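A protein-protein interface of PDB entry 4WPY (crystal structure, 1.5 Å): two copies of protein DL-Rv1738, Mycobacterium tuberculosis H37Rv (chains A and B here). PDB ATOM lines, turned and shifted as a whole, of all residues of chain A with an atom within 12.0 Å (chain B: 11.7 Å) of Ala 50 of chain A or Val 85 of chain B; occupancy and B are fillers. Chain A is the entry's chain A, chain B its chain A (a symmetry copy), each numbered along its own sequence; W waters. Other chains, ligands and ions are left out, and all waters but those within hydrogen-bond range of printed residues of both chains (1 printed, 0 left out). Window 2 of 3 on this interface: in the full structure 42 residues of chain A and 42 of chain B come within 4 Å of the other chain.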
ATOM      1  N   GLY A  24      19.886 -12.755 -13.812  1.00  0.00           N
ATOM      2  CA  GLY A  24      18.843 -13.660 -14.253  1.00  0.00           C
ATOM      3  C   GLY A  24      17.775 -13.974 -13.222  1.00  0.00           C
ATOM      4  O   GLY A  24      16.770 -14.616 -13.569  1.00  0.00           O
ATOM      5  N   ARG A  46      13.154 -16.673 -12.197  1.00  0.00           N
ATOM      6  CA  ARG A  46      14.494 -16.820 -12.738  1.00  0.00           C
ATOM      7  C   ARG A  46      14.401 -17.131 -14.215  1.00  0.00           C
ATOM      8  O   ARG A  46      13.643 -18.013 -14.615  1.00  0.00           O
ATOM      9  CB  ARG A  46      15.265 -17.913 -12.012  1.00  0.00           C
ATOM     10  CG  ARG A  46      16.752 -17.894 -12.452  1.00  0.00           C
ATOM     11  CD  ARG A  46      17.587 -18.811 -11.694  1.00  0.00           C
ATOM     12  NE  ARG A  46      17.746 -18.465 -10.293  1.00  0.00           N
ATOM     13  CZ  ARG A  46      18.737 -17.720  -9.807  1.00  0.00           C
ATOM     14  NH1 ARG A  46      19.649 -17.193 -10.618  1.00  0.00           N
ATOM     15  NH2 ARG A  46      18.799 -17.485  -8.497  1.00  0.00           N
ATOM     16  N   LEU A  47      15.148 -16.391 -15.016  1.00  0.00           N
ATOM     17  CA  LEU A  47      15.184 -16.644 -16.442  1.00  0.00           C
ATOM     18  C   LEU A  47      15.987 -17.899 -16.724  1.00  0.00           C
ATOM     19  O   LEU A  47      16.826 -18.333 -15.929  1.00  0.00           O
ATOM     20  CB  LEU A  47      15.799 -15.465 -17.185  1.00  0.00           C
ATOM     21  CG  LEU A  47      15.031 -14.152 -17.066  1.00  0.00           C
ATOM     22  CD1 LEU A  47      15.743 -13.061 -17.834  1.00  0.00           C
ATOM     23  CD2 LEU A  47      13.614 -14.294 -17.586  1.00  0.00           C
ATOM     24  N   ASN A  48      15.710 -18.490 -17.852  1.00  0.00           N
ATOM     25  CA  ASN A  48      16.503 -19.630 -18.264  1.00  0.00           C
ATOM     26  C   ASN A  48      17.139 -19.320 -19.606  1.00  0.00           C
ATOM     27  O   ASN A  48      16.861 -18.274 -20.200  1.00  0.00           O
ATOM     28  CB  ASN A  48      15.628 -20.870 -18.338  1.00  0.00           C
ATOM     29  CG  ASN A  48      14.551 -20.722 -19.317  1.00  0.00           C
ATOM     30  OD1 ASN A  48      14.796 -20.540 -20.509  1.00  0.00           O
ATOM     31  ND2 ASN A  48      13.343 -20.804 -18.853  1.00  0.00           N
ATOM     32  N   PRO A  49      17.999 -20.182 -20.109  1.00  0.00           N
ATOM     33  CA  PRO A  49      18.648 -19.893 -21.391  1.00  0.00           C
ATOM     34  C   PRO A  49      17.682 -19.580 -22.507  1.00  0.00           C
ATOM     35  O   PRO A  49      18.003 -18.754 -23.364  1.00  0.00           O
ATOM     36  CB  PRO A  49      19.443 -21.174 -21.660  1.00  0.00           C
ATOM     37  CG  PRO A  49      19.797 -21.648 -20.290  1.00  0.00           C
ATOM     38  CD  PRO A  49      18.579 -21.368 -19.457  1.00  0.00           C
ATOM     39  N   ALA A  50      16.496 -20.190 -22.519  1.00  0.00           N
ATOM     40  CA  ALA A  50      15.582 -19.964 -23.637  1.00  0.00           C
ATOM     41  C   ALA A  50      14.990 -18.560 -23.644  1.00  0.00           C
ATOM     42  O   ALA A  50      14.601 -18.066 -24.708  1.00  0.00           O
ATOM     43  CB  ALA A  50      14.453 -20.994 -23.611  1.00  0.00           C
ATOM     44  N   ASP A  51      14.851 -17.917 -22.487  1.00  0.00           N
ATOM     45  CA  ASP A  51      14.284 -16.570 -22.464  1.00  0.00           C
ATOM     46  C   ASP A  51      15.205 -15.590 -21.753  1.00  0.00           C
ATOM     47  O   ASP A  51      14.751 -14.541 -21.296  1.00  0.00           O
ATOM     48  CB  ASP A  51      12.876 -16.554 -21.856  1.00  0.00           C
ATOM     49  CG  ASP A  51      12.823 -17.007 -20.413  1.00  0.00           C
ATOM     50  OD1 ASP A  51      13.865 -17.219 -19.775  1.00  0.00           O
ATOM     51  OD2 ASP A  51      11.686 -17.146 -19.919  1.00  0.00           O
ATOM     52  N   ARG A  52      16.507 -15.886 -21.712  1.00  0.00           N
ATOM     53  CA  ARG A  52      17.417 -15.065 -20.927  1.00  0.00           C
ATOM     54  C   ARG A  52      17.492 -13.640 -21.446  1.00  0.00           C
ATOM     55  O   ARG A  52      17.828 -12.733 -20.677  1.00  0.00           O
ATOM     56  CB  ARG A  52      18.811 -15.700 -20.878  1.00  0.00           C
ATOM     57  CG  ARG A  52      19.696 -15.515 -22.024  1.00  0.00           C
ATOM     58  CD  ARG A  52      21.049 -16.200 -21.714  1.00  0.00           C
ATOM     59  NE  ARG A  52      21.984 -15.346 -20.984  1.00  0.00           N
ATOM     60  CZ  ARG A  52      23.207 -15.727 -20.618  1.00  0.00           C
ATOM     61  NH1 ARG A  52      24.004 -14.882 -19.984  1.00  0.00           N
ATOM     62  NH2 ARG A  52      23.635 -16.962 -20.879  1.00  0.00           N
ATOM     63  N   ASN A  53      17.158 -13.408 -22.713  1.00  0.00           N
ATOM     64  CA  ASN A  53      17.193 -12.069 -23.263  1.00  0.00           C
ATOM     65  C   ASN A  53      15.830 -11.395 -23.255  1.00  0.00           C
ATOM     66  O   ASN A  53      15.636 -10.415 -23.978  1.00  0.00           O
ATOM     67  CB  ASN A  53      17.746 -12.113 -24.679  1.00  0.00           C
ATOM     68  CG  ASN A  53      19.173 -12.594 -24.714  1.00  0.00           C
ATOM     69  OD1 ASN A  53      19.999 -12.181 -23.901  1.00  0.00           O
ATOM     70  ND2 ASN A  53      19.467 -13.489 -25.638  1.00  0.00           N
ATOM     71  N   VAL A  54      14.887 -11.893 -22.451  1.00  0.00           N
ATOM     72  CA  VAL A  54      13.550 -11.315 -22.357  1.00  0.00           C
ATOM     73  C   VAL A  54      13.286 -11.005 -20.891  1.00  0.00           C
ATOM     74  O   VAL A  54      12.470 -11.676 -20.235  1.00  0.00           O
ATOM     75  CB  VAL A  54      12.488 -12.257 -22.943  1.00  0.00           C
ATOM     76  CG1 VAL A  54      11.163 -11.505 -23.135  1.00  0.00           C
ATOM     77  CG2 VAL A  54      12.962 -12.810 -24.248  1.00  0.00           C
ATOM     78  N   PRO A  55      13.959 -10.004 -20.334  1.00  0.00           N
ATOM     79  CA  PRO A  55      13.793  -9.733 -18.897  1.00  0.00           C
ATOM     80  C   PRO A  55      12.378  -9.336 -18.535  1.00  0.00           C
ATOM     81  O   PRO A  55      11.993  -9.444 -17.359  1.00  0.00           O
ATOM     82  CB  PRO A  55      14.796  -8.602 -18.634  1.00  0.00           C
ATOM     83  CG  PRO A  55      15.068  -8.006 -19.984  1.00  0.00           C
ATOM     84  CD  PRO A  55      14.961  -9.126 -20.960  1.00  0.00           C
ATOM     85  N   GLU A  56      11.567  -8.937 -19.524  1.00  0.00           N
ATOM     86  CA  GLU A  56      10.191  -8.564 -19.234  1.00  0.00           C
ATOM     87  C   GLU A  56       9.408  -9.741 -18.684  1.00  0.00           C
ATOM     88  O   GLU A  56       8.475  -9.564 -17.886  1.00  0.00           O
ATOM     89  CB  GLU A  56       9.528  -8.012 -20.500  1.00  0.00           C
ATOM     90  CG  GLU A  56      10.292  -6.827 -21.094  1.00  0.00           C
ATOM     91  CD  GLU A  56      11.565  -7.174 -21.947  1.00  0.00           C
ATOM     92  OE1 GLU A  56      11.816  -8.329 -22.358  1.00  0.00           O
ATOM     93  OE2 GLU A  56      12.335  -6.230 -22.221  1.00  0.00           O
ATOM     94  N   ILE A  57       9.761 -10.950 -19.096  1.00  0.00           N
ATOM     95  CA  ILE A  57       9.111 -12.124 -18.545  1.00  0.00           C
ATOM     96  C   ILE A  57       9.424 -12.245 -17.057  1.00  0.00           C
ATOM     97  O   ILE A  57       8.539 -12.513 -16.246  1.00  0.00           O
ATOM     98  CB  ILE A  57       9.529 -13.379 -19.319  1.00  0.00           C
ATOM     99  CG1 ILE A  57       8.822 -13.393 -20.681  1.00  0.00           C
ATOM    100  CG2 ILE A  57       9.179 -14.623 -18.564  1.00  0.00           C
ATOM    101  CD1 ILE A  57       9.368 -14.384 -21.642  1.00  0.00           C
ATOM    102  N   GLY A  58      10.706 -12.116 -16.674  1.00  0.00           N
ATOM    103  CA  GLY A  58      11.023 -12.211 -15.249  1.00  0.00           C
ATOM    104  C   GLY A  58      10.326 -11.148 -14.428  1.00  0.00           C
ATOM    105  O   GLY A  58       9.888 -11.402 -13.293  1.00  0.00           O
ATOM    106  N   ASP A  59      10.207  -9.942 -14.988  1.00  0.00           N
ATOM    107  CA  ASP A  59       9.501  -8.874 -14.298  1.00  0.00           C
ATOM    108  C   ASP A  59       8.057  -9.260 -14.033  1.00  0.00           C
ATOM    109  O   ASP A  59       7.585  -9.218 -12.890  1.00  0.00           O
ATOM    110  CB  ASP A  59       9.530  -7.594 -15.117  1.00  0.00           C
ATOM    111  CG  ASP A  59      10.916  -7.040 -15.300  1.00  0.00           C
ATOM    112  OD1 ASP A  59      11.867  -7.472 -14.590  1.00  0.00           O
ATOM    113  OD2 ASP A  59      11.025  -6.134 -16.146  1.00  0.00           O
ATOM    114  N   GLU A  60       7.326  -9.608 -15.092  1.00  0.00           N
ATOM    115  CA  GLU A  60       5.898  -9.767 -14.929  1.00  0.00           C
ATOM    116  C   GLU A  60       5.578 -11.038 -14.168  1.00  0.00           C
ATOM    117  O   GLU A  60       4.597 -11.075 -13.415  1.00  0.00           O
ATOM    118  CB  GLU A  60       5.182  -9.731 -16.279  1.00  0.00           C
ATOM    119  CG  GLU A  60       5.476 -10.902 -17.174  1.00  0.00           C
ATOM    120  CD  GLU A  60       5.105 -10.669 -18.626  1.00  0.00           C
ATOM    121  OE1 GLU A  60       4.569  -9.584 -18.970  1.00  0.00           O
ATOM    122  OE2 GLU A  60       5.344 -11.599 -19.425  1.00  0.00           O
ATOM    123  N   LEU A  61       6.421 -12.057 -14.292  1.00  0.00           N
ATOM    124  CA  LEU A  61       6.172 -13.292 -13.573  1.00  0.00           C
ATOM    125  C   LEU A  61       6.459 -13.128 -12.080  1.00  0.00           C
ATOM    126  O   LEU A  61       5.689 -13.597 -11.236  1.00  0.00           O
ATOM    127  CB  LEU A  61       7.008 -14.408 -14.160  1.00  0.00           C
ATOM    128  CG  LEU A  61       6.817 -15.769 -13.523  1.00  0.00           C
ATOM    129  CD1 LEU A  61       5.344 -16.150 -13.390  1.00  0.00           C
ATOM    130  CD2 LEU A  61       7.622 -16.824 -14.319  1.00  0.00           C
ATOM    131  N   ARG B  35       4.578  -2.339 -19.319  1.00  0.00           N
ATOM    132  CA  ARG B  35       4.994  -2.470 -20.708  1.00  0.00           C
ATOM    133  C   ARG B  35       3.813  -2.418 -21.690  1.00  0.00           C
ATOM    134  O   ARG B  35       3.143  -1.388 -21.821  1.00  0.00           O
ATOM    135  CB  ARG B  35       5.800  -3.756 -20.834  1.00  0.00           C
ATOM    136  CG  ARG B  35       7.098  -3.769 -20.029  1.00  0.00           C
ATOM    137  CD  ARG B  35       8.284  -3.184 -20.759  1.00  0.00           C
ATOM    138  NE  ARG B  35       8.349  -3.651 -22.141  1.00  0.00           N
ATOM    139  CZ  ARG B  35       9.432  -3.663 -22.902  1.00  0.00           C
ATOM    140  NH1 ARG B  35      10.595  -3.251 -22.419  1.00  0.00           N
ATOM    141  NH2 ARG B  35       9.341  -4.106 -24.150  1.00  0.00           N
ATOM    142  N   GLU B  36       3.498  -3.530 -22.328  1.00  0.00           N
ATOM    143  CA  GLU B  36       2.483  -3.580 -23.373  1.00  0.00           C
ATOM    144  C   GLU B  36       1.166  -4.154 -22.900  1.00  0.00           C
ATOM    145  O   GLU B  36       0.369  -4.598 -23.734  1.00  0.00           O
ATOM    146  CB  GLU B  36       3.002  -4.418 -24.528  1.00  0.00           C
ATOM    147  CG  GLU B  36       4.200  -3.785 -25.177  1.00  0.00           C
ATOM    148  CD  GLU B  36       5.442  -4.588 -25.038  1.00  0.00           C
ATOM    149  OE1 GLU B  36       5.681  -5.196 -23.961  1.00  0.00           O
ATOM    150  OE2 GLU B  36       6.185  -4.588 -26.026  1.00  0.00           O
ATOM    151  N   LYS B  37       0.929  -4.190 -21.586  1.00  0.00           N
ATOM    152  CA  LYS B  37      -0.215  -4.911 -21.058  1.00  0.00           C
ATOM    153  C   LYS B  37      -0.961  -4.098 -20.010  1.00  0.00           C
ATOM    154  O   LYS B  37      -0.434  -3.154 -19.410  1.00  0.00           O
ATOM    155  CB  LYS B  37       0.206  -6.273 -20.480  1.00  0.00           C
ATOM    156  CG  LYS B  37       0.674  -7.254 -21.595  1.00  0.00           C
ATOM    157  CD  LYS B  37       2.105  -7.505 -21.453  1.00  0.00           C
ATOM    158  CE  LYS B  37       2.583  -8.412 -22.544  1.00  0.00           C
ATOM    159  NZ  LYS B  37       4.019  -8.662 -22.356  1.00  0.00           N
ATOM    160  N   LYS B  76      -1.296 -15.711 -16.485  1.00  0.00           N
ATOM    161  CA  LYS B  76      -1.699 -16.048 -17.852  1.00  0.00           C
ATOM    162  C   LYS B  76      -0.986 -15.183 -18.889  1.00  0.00           C
ATOM    163  O   LYS B  76      -0.532 -15.691 -19.920  1.00  0.00           O
ATOM    164  CB  LYS B  76      -3.212 -15.917 -18.006  1.00  0.00           C
ATOM    165  CG  LYS B  76      -3.974 -16.987 -17.291  1.00  0.00           C
ATOM    166  CD  LYS B  76      -5.462 -16.856 -17.569  1.00  0.00           C
ATOM    167  CE  LYS B  76      -6.261 -17.962 -16.897  1.00  0.00           C
ATOM    168  NZ  LYS B  76      -6.010 -17.991 -15.450  1.00  0.00           N
ATOM    169  N   VAL B  77      -0.876 -13.884 -18.652  1.00  0.00           N
ATOM    170  CA  VAL B  77      -0.107 -13.050 -19.569  1.00  0.00           C
ATOM    171  C   VAL B  77       1.331 -13.556 -19.661  1.00  0.00           C
ATOM    172  O   VAL B  77       1.901 -13.655 -20.759  1.00  0.00           O
ATOM    173  CB  VAL B  77      -0.151 -11.583 -19.129  1.00  0.00           C
ATOM    174  CG1 VAL B  77       0.720 -10.738 -20.060  1.00  0.00           C
ATOM    175  CG2 VAL B  77      -1.610 -11.083 -19.080  1.00  0.00           C
ATOM    176  N   SER B  78       1.946 -13.862 -18.508  1.00  0.00           N
ATOM    177  CA  SER B  78       3.316 -14.390 -18.494  1.00  0.00           C
ATOM    178  C   SER B  78       3.426 -15.641 -19.352  1.00  0.00           C
ATOM    179  O   SER B  78       4.386 -15.812 -20.131  1.00  0.00           O
ATOM    180  CB  SER B  78       3.749 -14.714 -17.057  1.00  0.00           C
ATOM    181  OG  SER B  78       3.774 -13.571 -16.234  1.00  0.00           O
ATOM    182  N   THR B  79       2.455 -16.535 -19.213  1.00  0.00           N
ATOM    183  CA  THR B  79       2.405 -17.726 -20.041  1.00  0.00           C
ATOM    184  C   THR B  79       2.414 -17.364 -21.516  1.00  0.00           C
ATOM    185  O   THR B  79       3.184 -17.925 -22.296  1.00  0.00           O
ATOM    186  CB  THR B  79       1.160 -18.529 -19.699  1.00  0.00           C
ATOM    187  OG1 THR B  79       1.216 -18.920 -18.323  1.00  0.00           O
ATOM    188  CG2 THR B  79       1.035 -19.752 -20.593  1.00  0.00           C
ATOM    189  N   HIS B  80       1.549 -16.427 -21.925  1.00  0.00           N
ATOM    190  CA  HIS B  80       1.495 -16.082 -23.339  1.00  0.00           C
ATOM    191  C   HIS B  80       2.832 -15.547 -23.825  1.00  0.00           C
ATOM    192  O   HIS B  80       3.258 -15.838 -24.959  1.00  0.00           O
ATOM    193  CB  HIS B  80       0.403 -15.053 -23.602  1.00  0.00           C
ATOM    194  CG  HIS B  80      -0.936 -15.479 -23.102  1.00  0.00           C
ATOM    195  ND1 HIS B  80      -1.890 -14.586 -22.677  1.00  0.00           N
ATOM    196  CD2 HIS B  80      -1.449 -16.712 -22.881  1.00  0.00           C
ATOM    197  CE1 HIS B  80      -2.944 -15.247 -22.231  1.00  0.00           C
ATOM    198  NE2 HIS B  80      -2.705 -16.540 -22.345  1.00  0.00           N
ATOM    199  N   ASP B  81       3.511 -14.765 -22.985  1.00  0.00           N
ATOM    200  CA  ASP B  81       4.788 -14.198 -23.388  1.00  0.00           C
ATOM    201  C   ASP B  81       5.866 -15.268 -23.474  1.00  0.00           C
ATOM    202  O   ASP B  81       6.707 -15.252 -24.386  1.00  0.00           O
ATOM    203  CB  ASP B  81       5.205 -13.109 -22.420  1.00  0.00           C
ATOM    204  CG  ASP B  81       4.389 -11.854 -22.572  1.00  0.00           C
ATOM    205  OD1 ASP B  81       3.641 -11.711 -23.579  1.00  0.00           O
ATOM    206  OD2 ASP B  81       4.532 -10.994 -21.700  1.00  0.00           O
ATOM    207  N   ILE B  82       5.862 -16.214 -22.544  1.00  0.00           N
ATOM    208  CA  ILE B  82       6.813 -17.315 -22.635  1.00  0.00           C
ATOM    209  C   ILE B  82       6.571 -18.117 -23.909  1.00  0.00           C
ATOM    210  O   ILE B  82       7.513 -18.484 -24.622  1.00  0.00           O
ATOM    211  CB  ILE B  82       6.702 -18.190 -21.382  1.00  0.00           C
ATOM    212  CG1 ILE B  82       7.235 -17.405 -20.194  1.00  0.00           C
ATOM    213  CG2 ILE B  82       7.469 -19.483 -21.571  1.00  0.00           C
ATOM    214  CD1 ILE B  82       6.834 -17.947 -18.839  1.00  0.00           C
ATOM    215  N   GLU B  83       5.305 -18.401 -24.208  1.00  0.00           N
ATOM    216  CA  GLU B  83       4.971 -19.149 -25.417  1.00  0.00           C
ATOM    217  C   GLU B  83       5.412 -18.407 -26.659  1.00  0.00           C
ATOM    218  O   GLU B  83       5.797 -19.031 -27.662  1.00  0.00           O
ATOM    219  CB  GLU B  83       3.462 -19.392 -25.489  1.00  0.00           C
ATOM    220  CG  GLU B  83       2.942 -20.338 -24.443  1.00  0.00           C
ATOM    221  CD  GLU B  83       1.428 -20.424 -24.440  1.00  0.00           C
ATOM    222  OE1 GLU B  83       0.747 -19.385 -24.599  1.00  0.00           O
ATOM    223  OE2 GLU B  83       0.911 -21.537 -24.272  1.00  0.00           O
ATOM    224  N   ALA B  84       5.336 -17.081 -26.636  1.00  0.00           N
ATOM    225  CA  ALA B  84       5.781 -16.323 -27.797  1.00  0.00           C
ATOM    226  C   ALA B  84       7.275 -16.480 -28.038  1.00  0.00           C
ATOM    227  O   ALA B  84       7.718 -16.442 -29.193  1.00  0.00           O
ATOM    228  CB  ALA B  84       5.427 -14.858 -27.635  1.00  0.00           C
ATOM    229  N   VAL B  85       8.060 -16.678 -26.979  1.00  0.00           N
ATOM    230  CA  VAL B  85       9.508 -16.850 -27.106  1.00  0.00           C
ATOM    231  C   VAL B  85       9.852 -18.275 -27.492  1.00  0.00           C
ATOM    232  O   VAL B  85      10.698 -18.508 -28.362  1.00  0.00           O
ATOM    233  CB  VAL B  85      10.208 -16.471 -25.788  1.00  0.00           C
ATOM    234  CG1 VAL B  85      11.716 -16.813 -25.861  1.00  0.00           C
ATOM    235  CG2 VAL B  85      10.000 -15.027 -25.493  1.00  0.00           C
ATOM    236  N   THR B  86       9.248 -19.251 -26.825  1.00  0.00           N
ATOM    237  CA  THR B  86       9.613 -20.647 -27.047  1.00  0.00           C
ATOM    238  C   THR B  86       8.884 -21.261 -28.231  1.00  0.00           C
ATOM    239  O   THR B  86       9.364 -22.259 -28.788  1.00  0.00           O
ATOM    240  CB  THR B  86       9.306 -21.480 -25.806  1.00  0.00           C
ATOM    241  OG1 THR B  86       7.881 -21.510 -25.598  1.00  0.00           O
ATOM    242  CG2 THR B  86       9.987 -20.887 -24.576  1.00  0.00           C
ATOM    243  N   HIS B  87       7.757 -20.677 -28.636  1.00  0.00           N
ATOM    244  CA  HIS B  87       6.892 -21.244 -29.668  1.00  0.00           C
ATOM    245  C   HIS B  87       6.415 -22.635 -29.278  1.00  0.00           C
ATOM    246  O   HIS B  87       6.212 -23.496 -30.137  1.00  0.00           O
ATOM    247  CB  HIS B  87       7.590 -21.279 -31.029  1.00  0.00           C
ATOM    248  CG  HIS B  87       8.275 -19.997 -31.382  1.00  0.00           C
ATOM    249  ND1 HIS B  87       7.585 -18.865 -31.752  1.00  0.00           N
ATOM    250  CD2 HIS B  87       9.588 -19.669 -31.428  1.00  0.00           C
ATOM    251  CE1 HIS B  87       8.440 -17.888 -31.994  1.00  0.00           C
ATOM    252  NE2 HIS B  87       9.663 -18.350 -31.809  1.00  0.00           N
ATOM    253  N   GLN B  88       6.267 -22.865 -27.976  1.00  0.00           N
ATOM    254  CA  GLN B  88       5.703 -24.088 -27.447  1.00  0.00           C
ATOM    255  C   GLN B  88       4.598 -23.733 -26.466  1.00  0.00           C
ATOM    256  O   GLN B  88       4.763 -22.799 -25.668  1.00  0.00           O
ATOM    257  CB  GLN B  88       6.760 -24.926 -26.734  1.00  0.00           C
ATOM    258  CG  GLN B  88       7.744 -25.571 -27.674  1.00  0.00           C
ATOM    259  CD  GLN B  88       8.583 -26.606 -26.972  1.00  0.00           C
ATOM    260  OE1 GLN B  88       9.620 -26.287 -26.386  1.00  0.00           O
ATOM    261  NE2 GLN B  88       8.131 -27.858 -27.007  1.00  0.00           N
ATOM    262  N   PRO B  89       3.471 -24.446 -26.494  1.00  0.00           N
ATOM    263  CA  PRO B  89       2.430 -24.197 -25.491  1.00  0.00           C
ATOM    264  C   PRO B  89       3.024 -24.259 -24.095  1.00  0.00           C
ATOM    265  O   PRO B  89       3.960 -25.017 -23.830  1.00  0.00           O
ATOM    266  CB  PRO B  89       1.428 -25.329 -25.727  1.00  0.00           C
ATOM    267  CG  PRO B  89       1.610 -25.695 -27.170  1.00  0.00           C
ATOM    268  CD  PRO B  89       3.089 -25.519 -27.431  1.00  0.00           C
ATOM    269  N   ALA B  90       2.497 -23.431 -23.205  1.00  0.00           N
ATOM    270  CA  ALA B  90       2.915 -23.489 -21.818  1.00  0.00           C
ATOM    271  C   ALA B  90       1.727 -23.173 -20.929  1.00  0.00           C
ATOM    272  O   ALA B  90       0.674 -22.690 -21.374  1.00  0.00           O
ATOM    273  CB  ALA B  90       4.070 -22.532 -21.512  1.00  0.00           C
ATOM    274  N   LEU B  92       1.467 -21.855 -16.691  1.00  0.00           N
ATOM    275  CA  LEU B  92       2.037 -21.602 -15.375  1.00  0.00           C
ATOM    276  C   LEU B  92       0.955 -21.797 -14.318  1.00  0.00           C
ATOM    277  O   LEU B  92      -0.092 -21.134 -14.347  1.00  0.00           O
ATOM    278  CB  LEU B  92       2.642 -20.202 -15.313  1.00  0.00           C
ATOM    279  CG  LEU B  92       4.028 -20.078 -15.963  1.00  0.00           C
ATOM    280  CD1 LEU B  92       4.033 -20.473 -17.436  1.00  0.00           C
ATOM    281  CD2 LEU B  92       4.524 -18.656 -15.807  1.00  0.00           C
HETATM  282  O   HOH W   1       5.901  -6.990 -20.778  1.00  0.00           O
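Among the printed residues, merely in contact across the chains: Ala 50 of chain A with Val 85 of chain B (3.4 Å), Val 54 of chain A with Val 85 of chain B (3.9 Å), Ile 57 of chain A with Asp 81 of chain B (3.9 Å), Ile 57 of chain A with Ile 82 of chain B (3.8 Å), Ile 57 of chain A with Val 85 of chain B (3.96 Å), Glu 60 of chain A with Ser 78 of chain B (3.3 Å), Leu 61 of chain A with Ser 78 of chain B (3.6 Å) and Leu 61 of chain A with Leu 92 of chain B (3.6 Å).
NZ of Lys 37 of chain B lies within salt-bridge range of OD2 of Asp 81 of chain B, at 2.5 Å.
OD1 of Asn 48 of chain A sits at hydrogen-bond distance from N of Ala 50 of chain A (2.7 Å).
O of Ile 82 of chain B lies within hydrogen-bond range of OG1 of Thr 86 of chain B (3.2 Å).
The guanidinium group of Arg 35 of chain B is in salt-bridge range of the side-chain carboxylate of Glu 36 of chain B, 3.6 Å away.
The side-chain hydroxyl (OG1) of Thr 79 of chain B lies close to the backbone NH (N) of Leu 92 of chain B (3.4 Å).
Printed residues of chain B that touch a printed residue of chain A: Arg 35, Lys 37, Ser 78, Asp 81, Ile 82, Val 85 and Leu 92.
Printed residues of chain A that touch a printed residue of chain B: Ala 50, Val 54, Glu 56, Ile 57, Glu 60 and Leu 61.
Hydrophobic or aromatic side chains of chain A that line the printed part of chain B: Val 54, Ile 57 and Leu 61.
Among the printed residues, Asp or Glu carboxylates within 4 Å of a Lys or Arg side-chain nitrogen of the other chain: Glu 56 of chain A with Arg 35 of chain B and Glu 60 of chain A with Lys 37 of chain B.
Water W1 lies within hydrogen-bond range of the side-chain amino group of Lys 37 of chain B (3.0 Å) and the side-chain carboxylate of Glu 60 of chain A (3.4 Å).
The side-chain carboxylate (OD2) of Asp 81 of chain B sits close to the side-chain carboxylate (OE2) of Glu 60 of chain A (2.5 Å).
OE2 of Glu 56 of chain A lies within salt-bridge range of NH1 of Arg 35 of chain B, 3.5 Å away.
NZ of Lys 37 of chain B is in salt-bridge range of OE1 of Glu 60 of chain A (3.6 Å).
Of the printed residues of chain B, Ala 50 of chain A touches Val 85.
Val 85 of chain B touches just these residues of chain A: Ala 50 (3.4 Å), Val 54 (3.9 Å) and Ile 57 (3.96 Å).
No residue of chain B comes within 4 Å of Asn 48 of chain A.
Pro 49 of chain A touches none of the printed residues of chain B.
No residue of chain B comes within 4 Å of Asp 51 of chain A.
Val 54 of chain A touches one residue of chain B.
Of chain A, only Ile 57 comes within 4 Å of Ile 82 of chain B.
No residue of chain A comes within 4 Å of Ala 84 of chain B.
Of the printed residues of chain B, Leu 61 of chain A touches Ser 78 and Leu 92.
Printed residues of chain B within 4 Å of Glu 60 of chain A: Lys 37 (3.6 Å), Ser 78 (3.3 Å) and Asp 81 (2.5 Å).
Printed residues of chain A within 4 Å of Ser 78 of chain B: Glu 60 (3.3 Å) and Leu 61 (3.6 Å).
Asp 59 of chain A touches none of the printed residues of chain B.
The nearest residue of chain A that does not touch Val 85 of chain B is Asp 51 of chain A (4.2 Å).
No position is printed for both chains.
Of the 11 pairs that touch across the chains among the printed residues, none has its exchanged pair printed and touching as well.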
